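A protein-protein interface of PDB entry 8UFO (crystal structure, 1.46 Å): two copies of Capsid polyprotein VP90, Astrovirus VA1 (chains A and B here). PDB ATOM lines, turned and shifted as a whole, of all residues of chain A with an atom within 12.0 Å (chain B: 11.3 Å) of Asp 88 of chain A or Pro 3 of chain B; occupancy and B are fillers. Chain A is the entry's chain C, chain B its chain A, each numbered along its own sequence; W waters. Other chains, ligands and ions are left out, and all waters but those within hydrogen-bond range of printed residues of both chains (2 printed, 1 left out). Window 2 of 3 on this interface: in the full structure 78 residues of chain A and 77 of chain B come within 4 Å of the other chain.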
ATOM      1  N   MET A   1      12.797 -11.570  29.694  1.00  0.00           N
ATOM      2  CA  MET A   1      11.461 -11.023  29.479  1.00  0.00           C
ATOM      3  C   MET A   1      10.438 -11.609  30.447  1.00  0.00           C
ATOM      4  O   MET A   1      10.295 -12.828  30.554  1.00  0.00           O
ATOM      5  CB  MET A   1      11.007 -11.258  28.033  1.00  0.00           C
ATOM      6  CG  MET A   1      11.451 -10.170  27.060  1.00  0.00           C
ATOM      7  SD  MET A   1      10.895 -10.418  25.355  1.00  0.00           S
ATOM      8  CE  MET A   1      12.000 -11.728  24.840  1.00  0.00           C
ATOM      9  N   ILE A   4       3.529  -9.989  29.769  1.00  0.00           N
ATOM     10  CA  ILE A   4       2.927  -8.719  29.370  1.00  0.00           C
ATOM     11  C   ILE A   4       1.599  -8.557  30.109  1.00  0.00           C
ATOM     12  O   ILE A   4       0.701  -9.396  29.934  1.00  0.00           O
ATOM     13  CB  ILE A   4       2.714  -8.665  27.854  1.00  0.00           C
ATOM     14  CG1 ILE A   4       4.063  -8.653  27.125  1.00  0.00           C
ATOM     15  CG2 ILE A   4       1.861  -7.470  27.472  1.00  0.00           C
ATOM     16  CD1 ILE A   4       3.945  -8.702  25.616  1.00  0.00           C
ATOM     17  N   PRO A  10      -9.346  -2.387  23.875  1.00  0.00           N
ATOM     18  CA  PRO A  10      -9.090  -2.853  22.509  1.00  0.00           C
ATOM     19  C   PRO A  10      -9.313  -1.736  21.502  1.00  0.00           C
ATOM     20  O   PRO A  10     -10.259  -0.950  21.612  1.00  0.00           O
ATOM     21  CB  PRO A  10     -10.116  -3.976  22.316  1.00  0.00           C
ATOM     22  CG  PRO A  10     -11.162  -3.740  23.358  1.00  0.00           C
ATOM     23  CD  PRO A  10     -10.445  -3.125  24.516  1.00  0.00           C
ATOM     24  N   VAL A  11      -8.425  -1.674  20.518  1.00  0.00           N
ATOM     25  CA  VAL A  11      -8.543  -0.762  19.391  1.00  0.00           C
ATOM     26  C   VAL A  11      -9.040  -1.583  18.210  1.00  0.00           C
ATOM     27  O   VAL A  11      -8.326  -2.456  17.705  1.00  0.00           O
ATOM     28  CB  VAL A  11      -7.205  -0.076  19.082  1.00  0.00           C
ATOM     29  CG1 VAL A  11      -7.320   0.797  17.839  1.00  0.00           C
ATOM     30  CG2 VAL A  11      -6.748   0.748  20.276  1.00  0.00           C
ATOM     31  N   GLY A  12     -10.273  -1.321  17.783  1.00  0.00           N
ATOM     32  CA  GLY A  12     -10.854  -2.050  16.682  1.00  0.00           C
ATOM     33  C   GLY A  12     -11.479  -3.362  17.124  1.00  0.00           C
ATOM     34  O   GLY A  12     -11.653  -3.635  18.315  1.00  0.00           O
ATOM     35  N   ASP A  13     -11.813  -4.183  16.129  1.00  0.00           N
ATOM     36  CA  ASP A  13     -12.438  -5.478  16.387  1.00  0.00           C
ATOM     37  C   ASP A  13     -11.528  -6.311  17.281  1.00  0.00           C
ATOM     38  O   ASP A  13     -10.300  -6.250  17.169  1.00  0.00           O
ATOM     39  CB  ASP A  13     -12.670  -6.196  15.059  1.00  0.00           C
ATOM     40  CG  ASP A  13     -13.660  -5.460  14.158  1.00  0.00           C
ATOM     41  OD1 ASP A  13     -14.254  -4.456  14.607  1.00  0.00           O
ATOM     42  OD2 ASP A  13     -13.807  -5.882  12.996  1.00  0.00           O
ATOM     43  N   PHE A  14     -12.124  -7.067  18.200  1.00  0.00           N
ATOM     44  CA  PHE A  14     -11.331  -7.678  19.262  1.00  0.00           C
ATOM     45  C   PHE A  14     -11.910  -9.025  19.674  1.00  0.00           C
ATOM     46  O   PHE A  14     -13.065  -9.367  19.377  1.00  0.00           O
ATOM     47  CB  PHE A  14     -11.229  -6.777  20.498  1.00  0.00           C
ATOM     48  CG  PHE A  14     -12.561  -6.428  21.116  1.00  0.00           C
ATOM     49  CD1 PHE A  14     -13.366  -5.431  20.574  1.00  0.00           C
ATOM     50  CD2 PHE A  14     -13.023  -7.129  22.223  1.00  0.00           C
ATOM     51  CE1 PHE A  14     -14.593  -5.119  21.150  1.00  0.00           C
ATOM     52  CE2 PHE A  14     -14.252  -6.830  22.795  1.00  0.00           C
ATOM     53  CZ  PHE A  14     -15.037  -5.826  22.261  1.00  0.00           C
ATOM     54  N   PHE A  15     -11.089  -9.777  20.403  1.00  0.00           N
ATOM     55  CA  PHE A  15     -11.456 -11.084  20.931  1.00  0.00           C
ATOM     56  C   PHE A  15     -11.598 -11.003  22.439  1.00  0.00           C
ATOM     57  O   PHE A  15     -10.896 -10.246  23.109  1.00  0.00           O
ATOM     58  CB  PHE A  15     -10.383 -12.131  20.626  1.00  0.00           C
ATOM     59  CG  PHE A  15     -10.197 -12.399  19.178  1.00  0.00           C
ATOM     60  CD1 PHE A  15      -9.510 -11.489  18.383  1.00  0.00           C
ATOM     61  CD2 PHE A  15     -10.700 -13.548  18.607  1.00  0.00           C
ATOM     62  CE1 PHE A  15      -9.329 -11.731  17.044  1.00  0.00           C
ATOM     63  CE2 PHE A  15     -10.528 -13.794  17.258  1.00  0.00           C
ATOM     64  CZ  PHE A  15      -9.833 -12.882  16.480  1.00  0.00           C
ATOM     65  N   VAL A  84      -8.539 -10.283  26.631  1.00  0.00           N
ATOM     66  CA  VAL A  84      -9.005  -9.427  25.546  1.00  0.00           C
ATOM     67  C   VAL A  84      -7.808  -9.129  24.655  1.00  0.00           C
ATOM     68  O   VAL A  84      -6.755  -8.713  25.154  1.00  0.00           O
ATOM     69  CB  VAL A  84      -9.597  -8.113  26.094  1.00  0.00           C
ATOM     70  CG1 VAL A  84     -10.087  -7.227  24.954  1.00  0.00           C
ATOM     71  CG2 VAL A  84     -10.705  -8.400  27.110  1.00  0.00           C
ATOM     72  N   TRP A  85      -7.958  -9.320  23.344  1.00  0.00           N
ATOM     73  CA  TRP A  85      -6.817  -9.040  22.478  1.00  0.00           C
ATOM     74  C   TRP A  85      -7.266  -8.610  21.094  1.00  0.00           C
ATOM     75  O   TRP A  85      -8.407  -8.838  20.680  1.00  0.00           O
ATOM     76  CB  TRP A  85      -5.847 -10.226  22.394  1.00  0.00           C
ATOM     77  CG  TRP A  85      -6.353 -11.423  21.632  1.00  0.00           C
ATOM     78  CD1 TRP A  85      -6.248 -11.649  20.295  1.00  0.00           C
ATOM     79  CD2 TRP A  85      -7.012 -12.577  22.178  1.00  0.00           C
ATOM     80  NE1 TRP A  85      -6.807 -12.864  19.968  1.00  0.00           N
ATOM     81  CE2 TRP A  85      -7.273 -13.455  21.113  1.00  0.00           C
ATOM     82  CE3 TRP A  85      -7.395 -12.947  23.470  1.00  0.00           C
ATOM     83  CZ2 TRP A  85      -7.928 -14.675  21.293  1.00  0.00           C
ATOM     84  CZ3 TRP A  85      -8.039 -14.165  23.649  1.00  0.00           C
ATOM     85  CH2 TRP A  85      -8.294 -15.009  22.569  1.00  0.00           C
ATOM     86  N   THR A  86      -6.334  -7.991  20.372  1.00  0.00           N
ATOM     87  CA  THR A  86      -6.525  -7.687  18.964  1.00  0.00           C
ATOM     88  C   THR A  86      -5.378  -8.280  18.159  1.00  0.00           C
ATOM     89  O   THR A  86      -4.269  -8.482  18.679  1.00  0.00           O
ATOM     90  CB  THR A  86      -6.619  -6.173  18.716  1.00  0.00           C
ATOM     91  OG1 THR A  86      -5.409  -5.535  19.167  1.00  0.00           O
ATOM     92  CG2 THR A  86      -7.825  -5.583  19.465  1.00  0.00           C
ATOM     93  N   LEU A  87      -5.657  -8.549  16.883  1.00  0.00           N
ATOM     94  CA  LEU A  87      -4.722  -9.183  15.970  1.00  0.00           C
ATOM     95  C   LEU A  87      -4.474  -8.297  14.760  1.00  0.00           C
ATOM     96  O   LEU A  87      -5.369  -7.582  14.296  1.00  0.00           O
ATOM     97  CB  LEU A  87      -5.285 -10.502  15.440  1.00  0.00           C
ATOM     98  CG  LEU A  87      -5.577 -11.591  16.472  1.00  0.00           C
ATOM     99  CD1 LEU A  87      -6.165 -12.802  15.767  1.00  0.00           C
ATOM    100  CD2 LEU A  87      -4.305 -11.973  17.239  1.00  0.00           C
ATOM    101  N   ASP A  88      -3.248  -8.379  14.245  1.00  0.00           N
ATOM    102  CA  ASP A  88      -2.858  -7.882  12.926  1.00  0.00           C
ATOM    103  C   ASP A  88      -2.442  -9.127  12.146  1.00  0.00           C
ATOM    104  O   ASP A  88      -1.296  -9.568  12.228  1.00  0.00           O
ATOM    105  CB  ASP A  88      -1.707  -6.878  13.072  1.00  0.00           C
ATOM    106  CG  ASP A  88      -1.188  -6.371  11.735  1.00  0.00           C
ATOM    107  OD1 ASP A  88      -1.884  -6.522  10.710  1.00  0.00           O
ATOM    108  OD2 ASP A  88      -0.073  -5.813  11.717  1.00  0.00           O
ATOM    109  N   GLY A  89      -3.379  -9.710  11.404  1.00  0.00           N
ATOM    110  CA  GLY A  89      -3.151 -11.021  10.831  1.00  0.00           C
ATOM    111  C   GLY A  89      -3.039 -12.060  11.930  1.00  0.00           C
ATOM    112  O   GLY A  89      -3.971 -12.228  12.722  1.00  0.00           O
ATOM    113  N   GLN A  90      -1.907 -12.753  11.997  1.00  0.00           N
ATOM    114  CA  GLN A  90      -1.625 -13.659  13.105  1.00  0.00           C
ATOM    115  C   GLN A  90      -0.824 -12.990  14.219  1.00  0.00           C
ATOM    116  O   GLN A  90      -0.564 -13.625  15.247  1.00  0.00           O
ATOM    117  CB  GLN A  90      -0.896 -14.910  12.604  1.00  0.00           C
ATOM    118  CG  GLN A  90      -1.664 -15.667  11.518  1.00  0.00           C
ATOM    119  CD  GLN A  90      -3.027 -16.153  11.997  1.00  0.00           C
ATOM    120  OE1 GLN A  90      -3.132 -16.885  12.982  1.00  0.00           O
ATOM    121  NE2 GLN A  90      -4.080 -15.727  11.306  1.00  0.00           N
ATOM    122  N   LYS A  91      -0.448 -11.726  14.049  1.00  0.00           N
ATOM    123  CA  LYS A  91       0.382 -11.027  15.015  1.00  0.00           C
ATOM    124  C   LYS A  91      -0.493 -10.436  16.110  1.00  0.00           C
ATOM    125  O   LYS A  91      -1.592  -9.942  15.846  1.00  0.00           O
ATOM    126  CB  LYS A  91       1.118  -9.882  14.316  1.00  0.00           C
ATOM    127  CG  LYS A  91       2.057 -10.350  13.224  1.00  0.00           C
ATOM    128  CD  LYS A  91       2.745  -9.156  12.596  1.00  0.00           C
ATOM    129  CE  LYS A  91       3.705  -9.592  11.510  1.00  0.00           C
ATOM    130  NZ  LYS A  91       4.077  -8.439  10.650  1.00  0.00           N
ATOM    131  N   LEU A  92       0.004 -10.482  17.340  1.00  0.00           N
ATOM    132  CA  LEU A  92      -0.706  -9.906  18.472  1.00  0.00           C
ATOM    133  C   LEU A  92      -0.489  -8.399  18.479  1.00  0.00           C
ATOM    134  O   LEU A  92       0.645  -7.934  18.643  1.00  0.00           O
ATOM    135  CB  LEU A  92      -0.174 -10.520  19.760  1.00  0.00           C
ATOM    136  CG  LEU A  92      -0.933 -10.028  20.982  1.00  0.00           C
ATOM    137  CD1 LEU A  92      -2.360 -10.601  21.031  1.00  0.00           C
ATOM    138  CD2 LEU A  92      -0.160 -10.397  22.203  1.00  0.00           C
ATOM    139  N   SER A  93      -1.560  -7.630  18.313  1.00  0.00           N
ATOM    140  CA  SER A  93      -1.431  -6.175  18.291  1.00  0.00           C
ATOM    141  C   SER A  93      -1.849  -5.496  19.591  1.00  0.00           C
ATOM    142  O   SER A  93      -1.523  -4.318  19.797  1.00  0.00           O
ATOM    143  CB  SER A  93      -2.177  -5.580  17.092  1.00  0.00           C
ATOM    144  OG  SER A  93      -3.565  -5.858  17.155  1.00  0.00           O
ATOM    145  N   GLY A  94      -2.541  -6.200  20.477  1.00  0.00           N
ATOM    146  CA  GLY A  94      -2.921  -5.633  21.749  1.00  0.00           C
ATOM    147  C   GLY A  94      -3.282  -6.729  22.727  1.00  0.00           C
ATOM    148  O   GLY A  94      -3.907  -7.724  22.338  1.00  0.00           O
ATOM    149  N   TRP A  95      -2.868  -6.574  23.981  1.00  0.00           N
ATOM    150  CA  TRP A  95      -3.260  -7.473  25.065  1.00  0.00           C
ATOM    151  C   TRP A  95      -3.936  -6.553  26.066  1.00  0.00           C
ATOM    152  O   TRP A  95      -3.259  -5.830  26.801  1.00  0.00           O
ATOM    153  CB  TRP A  95      -2.041  -8.167  25.674  1.00  0.00           C
ATOM    154  CG  TRP A  95      -2.403  -9.299  26.602  1.00  0.00           C
ATOM    155  CD1 TRP A  95      -2.221  -9.343  27.962  1.00  0.00           C
ATOM    156  CD2 TRP A  95      -2.998 -10.553  26.235  1.00  0.00           C
ATOM    157  NE1 TRP A  95      -2.669 -10.548  28.460  1.00  0.00           N
ATOM    158  CE2 TRP A  95      -3.142 -11.311  27.422  1.00  0.00           C
ATOM    159  CE3 TRP A  95      -3.396 -11.120  25.018  1.00  0.00           C
ATOM    160  CZ2 TRP A  95      -3.690 -12.594  27.426  1.00  0.00           C
ATOM    161  CZ3 TRP A  95      -3.947 -12.395  25.023  1.00  0.00           C
ATOM    162  CH2 TRP A  95      -4.079 -13.117  26.223  1.00  0.00           C
ATOM    163  N   ASN A  96      -5.270  -6.553  26.073  1.00  0.00           N
ATOM    164  CA  ASN A  96      -6.054  -5.419  26.541  1.00  0.00           C
ATOM    165  C   ASN A  96      -6.964  -5.822  27.697  1.00  0.00           C
ATOM    166  O   ASN A  96      -6.939  -6.951  28.177  1.00  0.00           O
ATOM    167  CB  ASN A  96      -6.888  -4.857  25.382  1.00  0.00           C
ATOM    168  CG  ASN A  96      -6.027  -4.364  24.233  1.00  0.00           C
ATOM    169  OD1 ASN A  96      -6.200  -4.785  23.089  1.00  0.00           O
ATOM    170  ND2 ASN A  96      -5.055  -3.505  24.547  1.00  0.00           N
ATOM    171  N   HIS A 271     -15.522 -13.200  19.148  1.00  0.00           N
ATOM    172  CA  HIS A 271     -14.899 -12.099  18.429  1.00  0.00           C
ATOM    173  C   HIS A 271     -15.967 -11.058  18.160  1.00  0.00           C
ATOM    174  O   HIS A 271     -17.107 -11.399  17.830  1.00  0.00           O
ATOM    175  CB  HIS A 271     -14.299 -12.595  17.110  1.00  0.00           C
ATOM    176  CG  HIS A 271     -13.710 -11.511  16.265  1.00  0.00           C
ATOM    177  ND1 HIS A 271     -14.107 -11.271  14.967  1.00  0.00           N
ATOM    178  CD2 HIS A 271     -12.718 -10.624  16.523  1.00  0.00           C
ATOM    179  CE1 HIS A 271     -13.403 -10.270  14.470  1.00  0.00           C
ATOM    180  NE2 HIS A 271     -12.551  -9.860  15.393  1.00  0.00           N
ATOM    181  N   MET B   1       4.313  -1.565  22.617  1.00  0.00           N
ATOM    182  CA  MET B   1       4.974  -2.548  21.769  1.00  0.00           C
ATOM    183  C   MET B   1       4.238  -2.694  20.437  1.00  0.00           C
ATOM    184  O   MET B   1       3.008  -2.695  20.407  1.00  0.00           O
ATOM    185  CB  MET B   1       5.008  -3.895  22.483  1.00  0.00           C
ATOM    186  CG  MET B   1       6.052  -4.849  21.967  1.00  0.00           C
ATOM    187  SD  MET B   1       6.800  -5.644  23.386  1.00  0.00           S
ATOM    188  CE  MET B   1       7.652  -4.225  24.036  1.00  0.00           C
ATOM    189  N   GLY B   2       4.994  -2.812  19.340  1.00  0.00           N
ATOM    190  CA  GLY B   2       4.425  -3.082  18.034  1.00  0.00           C
ATOM    191  C   GLY B   2       3.939  -4.517  17.949  1.00  0.00           C
ATOM    192  O   GLY B   2       4.208  -5.320  18.845  1.00  0.00           O
ATOM    193  N   PRO B   3       3.226  -4.875  16.874  1.00  0.00           N
ATOM    194  CA  PRO B   3       2.586  -6.200  16.832  1.00  0.00           C
ATOM    195  C   PRO B   3       3.606  -7.330  16.845  1.00  0.00           C
ATOM    196  O   PRO B   3       4.638  -7.279  16.171  1.00  0.00           O
ATOM    197  CB  PRO B   3       1.782  -6.179  15.525  1.00  0.00           C
ATOM    198  CG  PRO B   3       1.688  -4.738  15.138  1.00  0.00           C
ATOM    199  CD  PRO B   3       2.935  -4.090  15.663  1.00  0.00           C
ATOM    200  N   ILE B   4       3.297  -8.367  17.615  1.00  0.00           N
ATOM    201  CA  ILE B   4       4.239  -9.446  17.905  1.00  0.00           C
ATOM    202  C   ILE B   4       3.879 -10.651  17.039  1.00  0.00           C
ATOM    203  O   ILE B   4       2.781 -11.204  17.195  1.00  0.00           O
ATOM    204  CB  ILE B   4       4.206  -9.818  19.393  1.00  0.00           C
ATOM    205  CG1 ILE B   4       4.624  -8.620  20.257  1.00  0.00           C
ATOM    206  CG2 ILE B   4       5.113 -11.025  19.653  1.00  0.00           C
ATOM    207  CD1 ILE B   4       4.864  -8.963  21.718  1.00  0.00           C
ATOM    208  N   PRO B   5       4.768 -11.111  16.159  1.00  0.00           N
ATOM    209  CA  PRO B   5       4.463 -12.310  15.385  1.00  0.00           C
ATOM    210  C   PRO B   5       4.502 -13.536  16.276  1.00  0.00           C
ATOM    211  O   PRO B   5       5.221 -13.565  17.289  1.00  0.00           O
ATOM    212  CB  PRO B   5       5.593 -12.350  14.342  1.00  0.00           C
ATOM    213  CG  PRO B   5       6.726 -11.655  15.011  1.00  0.00           C
ATOM    214  CD  PRO B   5       6.124 -10.595  15.889  1.00  0.00           C
ATOM    215  N   PRO B   6       3.742 -14.580  15.940  1.00  0.00           N
ATOM    216  CA  PRO B   6       3.858 -15.831  16.699  1.00  0.00           C
ATOM    217  C   PRO B   6       5.279 -16.354  16.589  1.00  0.00           C
ATOM    218  O   PRO B   6       5.851 -16.429  15.498  1.00  0.00           O
ATOM    219  CB  PRO B   6       2.852 -16.762  16.016  1.00  0.00           C
ATOM    220  CG  PRO B   6       2.596 -16.148  14.668  1.00  0.00           C
ATOM    221  CD  PRO B   6       2.781 -14.676  14.828  1.00  0.00           C
ATOM    222  N   THR B   7       5.855 -16.692  17.736  1.00  0.00           N
ATOM    223  CA  THR B   7       7.291 -16.920  17.827  1.00  0.00           C
ATOM    224  C   THR B   7       7.539 -17.943  18.918  1.00  0.00           C
ATOM    225  O   THR B   7       7.137 -17.733  20.066  1.00  0.00           O
ATOM    226  CB  THR B   7       7.982 -15.600  18.177  1.00  0.00           C
ATOM    227  OG1 THR B   7       7.702 -14.639  17.150  1.00  0.00           O
ATOM    228  CG2 THR B   7       9.485 -15.785  18.302  1.00  0.00           C
ATOM    229  N   SER B  80      -1.243 -23.076  10.813  1.00  0.00           N
ATOM    230  CA  SER B  80      -1.116 -21.708  10.324  1.00  0.00           C
ATOM    231  C   SER B  80      -2.316 -20.842  10.675  1.00  0.00           C
ATOM    232  O   SER B  80      -2.227 -19.615  10.548  1.00  0.00           O
ATOM    233  CB  SER B  80      -0.905 -21.716   8.811  1.00  0.00           C
ATOM    234  OG  SER B  80      -2.104 -22.057   8.138  1.00  0.00           O
ATOM    235  N   GLU B  81      -3.424 -21.446  11.109  1.00  0.00           N
ATOM    236  CA  GLU B  81      -4.658 -20.740  11.432  1.00  0.00           C
ATOM    237  C   GLU B  81      -5.090 -20.982  12.877  1.00  0.00           C
ATOM    238  O   GLU B  81      -6.284 -20.994  13.184  1.00  0.00           O
ATOM    239  CB  GLU B  81      -5.777 -21.139  10.463  1.00  0.00           C
ATOM    240  CG  GLU B  81      -5.583 -20.673   9.019  1.00  0.00           C
ATOM    241  CD  GLU B  81      -5.160 -19.219   8.917  1.00  0.00           C
ATOM    242  OE1 GLU B  81      -5.877 -18.347   9.456  1.00  0.00           O
ATOM    243  OE2 GLU B  81      -4.113 -18.946   8.291  1.00  0.00           O
ATOM    244  N   ALA B  82      -4.134 -21.189  13.776  1.00  0.00           N
ATOM    245  CA  ALA B  82      -4.421 -21.323  15.197  1.00  0.00           C
ATOM    246  C   ALA B  82      -3.652 -20.265  15.972  1.00  0.00           C
ATOM    247  O   ALA B  82      -2.498 -19.969  15.648  1.00  0.00           O
ATOM    248  CB  ALA B  82      -4.003 -22.702  15.716  1.00  0.00           C
ATOM    249  N   LEU B  83      -4.302 -19.701  16.987  1.00  0.00           N
ATOM    250  CA  LEU B  83      -3.637 -18.847  17.960  1.00  0.00           C
ATOM    251  C   LEU B  83      -3.138 -19.727  19.098  1.00  0.00           C
ATOM    252  O   LEU B  83      -3.855 -20.615  19.567  1.00  0.00           O
ATOM    253  CB  LEU B  83      -4.621 -17.810  18.500  1.00  0.00           C
ATOM    254  CG  LEU B  83      -5.397 -17.040  17.425  1.00  0.00           C
ATOM    255  CD1 LEU B  83      -6.360 -16.075  18.079  1.00  0.00           C
ATOM    256  CD2 LEU B  83      -4.422 -16.311  16.495  1.00  0.00           C
ATOM    257  N   LEU B  92       0.373 -12.129  29.592  1.00  0.00           N
ATOM    258  CA  LEU B  92       0.760 -12.929  28.440  1.00  0.00           C
ATOM    259  C   LEU B  92       2.240 -13.281  28.542  1.00  0.00           C
ATOM    260  O   LEU B  92       3.098 -12.393  28.506  1.00  0.00           O
ATOM    261  CB  LEU B  92       0.488 -12.131  27.171  1.00  0.00           C
ATOM    262  CG  LEU B  92       0.869 -12.917  25.933  1.00  0.00           C
ATOM    263  CD1 LEU B  92      -0.237 -13.896  25.585  1.00  0.00           C
ATOM    264  CD2 LEU B  92       1.107 -11.949  24.819  1.00  0.00           C
ATOM    265  N   TRP B  95       3.516 -15.654  22.905  1.00  0.00           N
ATOM    266  CA  TRP B  95       2.644 -15.614  21.731  1.00  0.00           C
ATOM    267  C   TRP B  95       3.333 -16.524  20.731  1.00  0.00           C
ATOM    268  O   TRP B  95       4.317 -16.131  20.098  1.00  0.00           O
ATOM    269  CB  TRP B  95       2.505 -14.186  21.190  1.00  0.00           C
ATOM    270  CG  TRP B  95       1.461 -14.074  20.110  1.00  0.00           C
ATOM    271  CD1 TRP B  95       1.667 -13.832  18.781  1.00  0.00           C
ATOM    272  CD2 TRP B  95       0.048 -14.260  20.265  1.00  0.00           C
ATOM    273  NE1 TRP B  95       0.467 -13.812  18.108  1.00  0.00           N
ATOM    274  CE2 TRP B  95      -0.544 -14.076  18.993  1.00  0.00           C
ATOM    275  CE3 TRP B  95      -0.774 -14.522  21.361  1.00  0.00           C
ATOM    276  CZ2 TRP B  95      -1.919 -14.172  18.784  1.00  0.00           C
ATOM    277  CZ3 TRP B  95      -2.136 -14.622  21.160  1.00  0.00           C
ATOM    278  CH2 TRP B  95      -2.701 -14.440  19.877  1.00  0.00           C
ATOM    279  N   ASN B  96       2.831 -17.747  20.601  1.00  0.00           N
ATOM    280  CA  ASN B  96       3.646 -18.863  20.143  1.00  0.00           C
ATOM    281  C   ASN B  96       3.095 -19.466  18.859  1.00  0.00           C
ATOM    282  O   ASN B  96       2.068 -19.047  18.329  1.00  0.00           O
ATOM    283  CB  ASN B  96       3.731 -19.939  21.234  1.00  0.00           C
ATOM    284  CG  ASN B  96       4.401 -19.442  22.492  1.00  0.00           C
ATOM    285  OD1 ASN B  96       3.851 -19.545  23.585  1.00  0.00           O
ATOM    286  ND2 ASN B  96       5.589 -18.864  22.341  1.00  0.00           N
HETATM  287  O   HOH W   1       5.443  -7.207  13.472  1.00  0.00           O
HETATM  288  O   HOH W   2       0.854  -3.459  18.585  1.00  0.00           O
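The backbone carbonyl oxygen (O) of Gln 90 of chain A is in hydrogen-bond range of the indole nitrogen (NE1) of Trp 95 of chain B, 3.0 Å away. N of Leu 92 of chain A is in hydrogen-bond range of O of Ile 4 of chain B (2.9 Å). The indole nitrogen of Trp 95 of chain B lies close to the backbone NH of Leu 92 of chain A (3.4 Å). The backbone NH (N) of Ile 4 of chain A lies within hydrogen-bond range of the backbone carbonyl oxygen (O) of Leu 92 of chain B.
The side-chain hydroxyl (OG1) of Thr 7 of chain B is in hydrogen-bond range of the backbone carbonyl oxygen (O) of Pro 5 of chain B, at 2.7 Å. The backbone NH (N) of Phe 15 of chain A sits at hydrogen-bond distance from the backbone carbonyl oxygen (O) of Trp 85 of chain A, at 2.9 Å. N of Leu 87 of chain A sits at hydrogen-bond distance from OG of Ser 93 of chain A (3.4 Å). N of Thr 7 of chain B lies within hydrogen-bond range of O of Trp 95 of chain B (2.9 Å).
Among the printed residues, merely in contact across the chains: Trp 85 of chain A with Leu 83 of chain B (3.8 Å), Leu 87 of chain A with Leu 83 of chain B (3.99 Å), Leu 87 of chain A with Trp 95 of chain B (3.6 Å), Asp 88 of chain A with Pro 3 of chain B (3.99 Å), Gln 90 of chain A with Pro 6 of chain B (3.5 Å), Gln 90 of chain A with Ser 80 of chain B (3.8 Å), Gln 90 of chain A with Glu 81 of chain B (3.7 Å), Gln 90 of chain A with Leu 83 of chain B (3.8 Å), Lys 91 of chain A with Pro 3 of chain B (3.95 Å), Lys 91 of chain A with Ile 4 of chain B (3.2 Å), Lys 91 of chain A with Pro 5 of chain B (3.8 Å), Leu 92 of chain A with Pro 3 of chain B (3.2 Å), Leu 92 of chain A with Leu 92 of chain B (3.3 Å) and Trp 95 of chain A with Leu 92 of chain B (3.6 Å).
Printed residues of chain B within 4 Å of Asp 88 of chain A: Pro 3. Of the printed residues of chain A, Pro 3 of chain B touches Asp 88 (3.99 Å), Lys 91 (3.95 Å) and Leu 92 (3.2 Å). No residue of chain B comes within 4 Å of Gly 89 of chain A. Of chain B, only Pro 3, Ile 4 and Pro 5 come within 4 Å of Lys 91 of chain A. Leu 92 of chain A touches just these residues of chain B: Pro 3 (3.2 Å), Ile 4 (2.9 Å), Leu 92 (3.3 Å) and Trp 95 (3.4 Å). No residue of chain B comes within 4 Å of Ser 93 of chain A. Of chain A, only Lys 91 (3.8 Å) comes within 4 Å of Pro 5 of chain B. Of the printed residues of chain A, Glu 81 of chain B touches Gln 90 (3.7 Å). Of the printed residues of chain A, Leu 92 of chain B touches Ile 4, Leu 92 and Trp 95. The nearest printed residue of chain B that does not touch Asp 88 of chain A is Ile 4 of chain B (6.6 Å).
Water W2 bridges the backbone carbonyl oxygen of Ser 93 of chain A (2.8 Å) and the backbone carbonyl oxygen of Met 1 of chain B (2.9 Å). Water W1 lies within hydrogen-bond range of the backbone carbonyl oxygen of Pro 3 of chain B (2.8 Å) and the side-chain amino group of Lys 91 of chain A (3.4 Å).
Ile 4 of chain A touches Leu 92 of chain B, and with the chains exchanged Leu 92 of chain A touches Ile 4 of chain B. Leu 92 of chain B touches its own counterpart, Leu 92 of chain A. Leu 92 of chain A touches Trp 95 of chain B, and with the chains exchanged Trp 95 of chain A touches Leu 92 of chain B. Positions printed for both chains: 1, 4, 92, 95 and 96. Of the 18 pairs that touch across the chains among the printed residues, 5 have their exchanged pair printed and touching as well.
Hydrophobic or aromatic side chains of chain B within 4 Å of the printed part of chain A: Pro 3, Pro 6, Leu 83, Leu 92 and Trp 95. Among the printed residues, no Asp or Glu carboxylate lies within 4 Å of a Lys or Arg side-chain nitrogen of the other chain.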
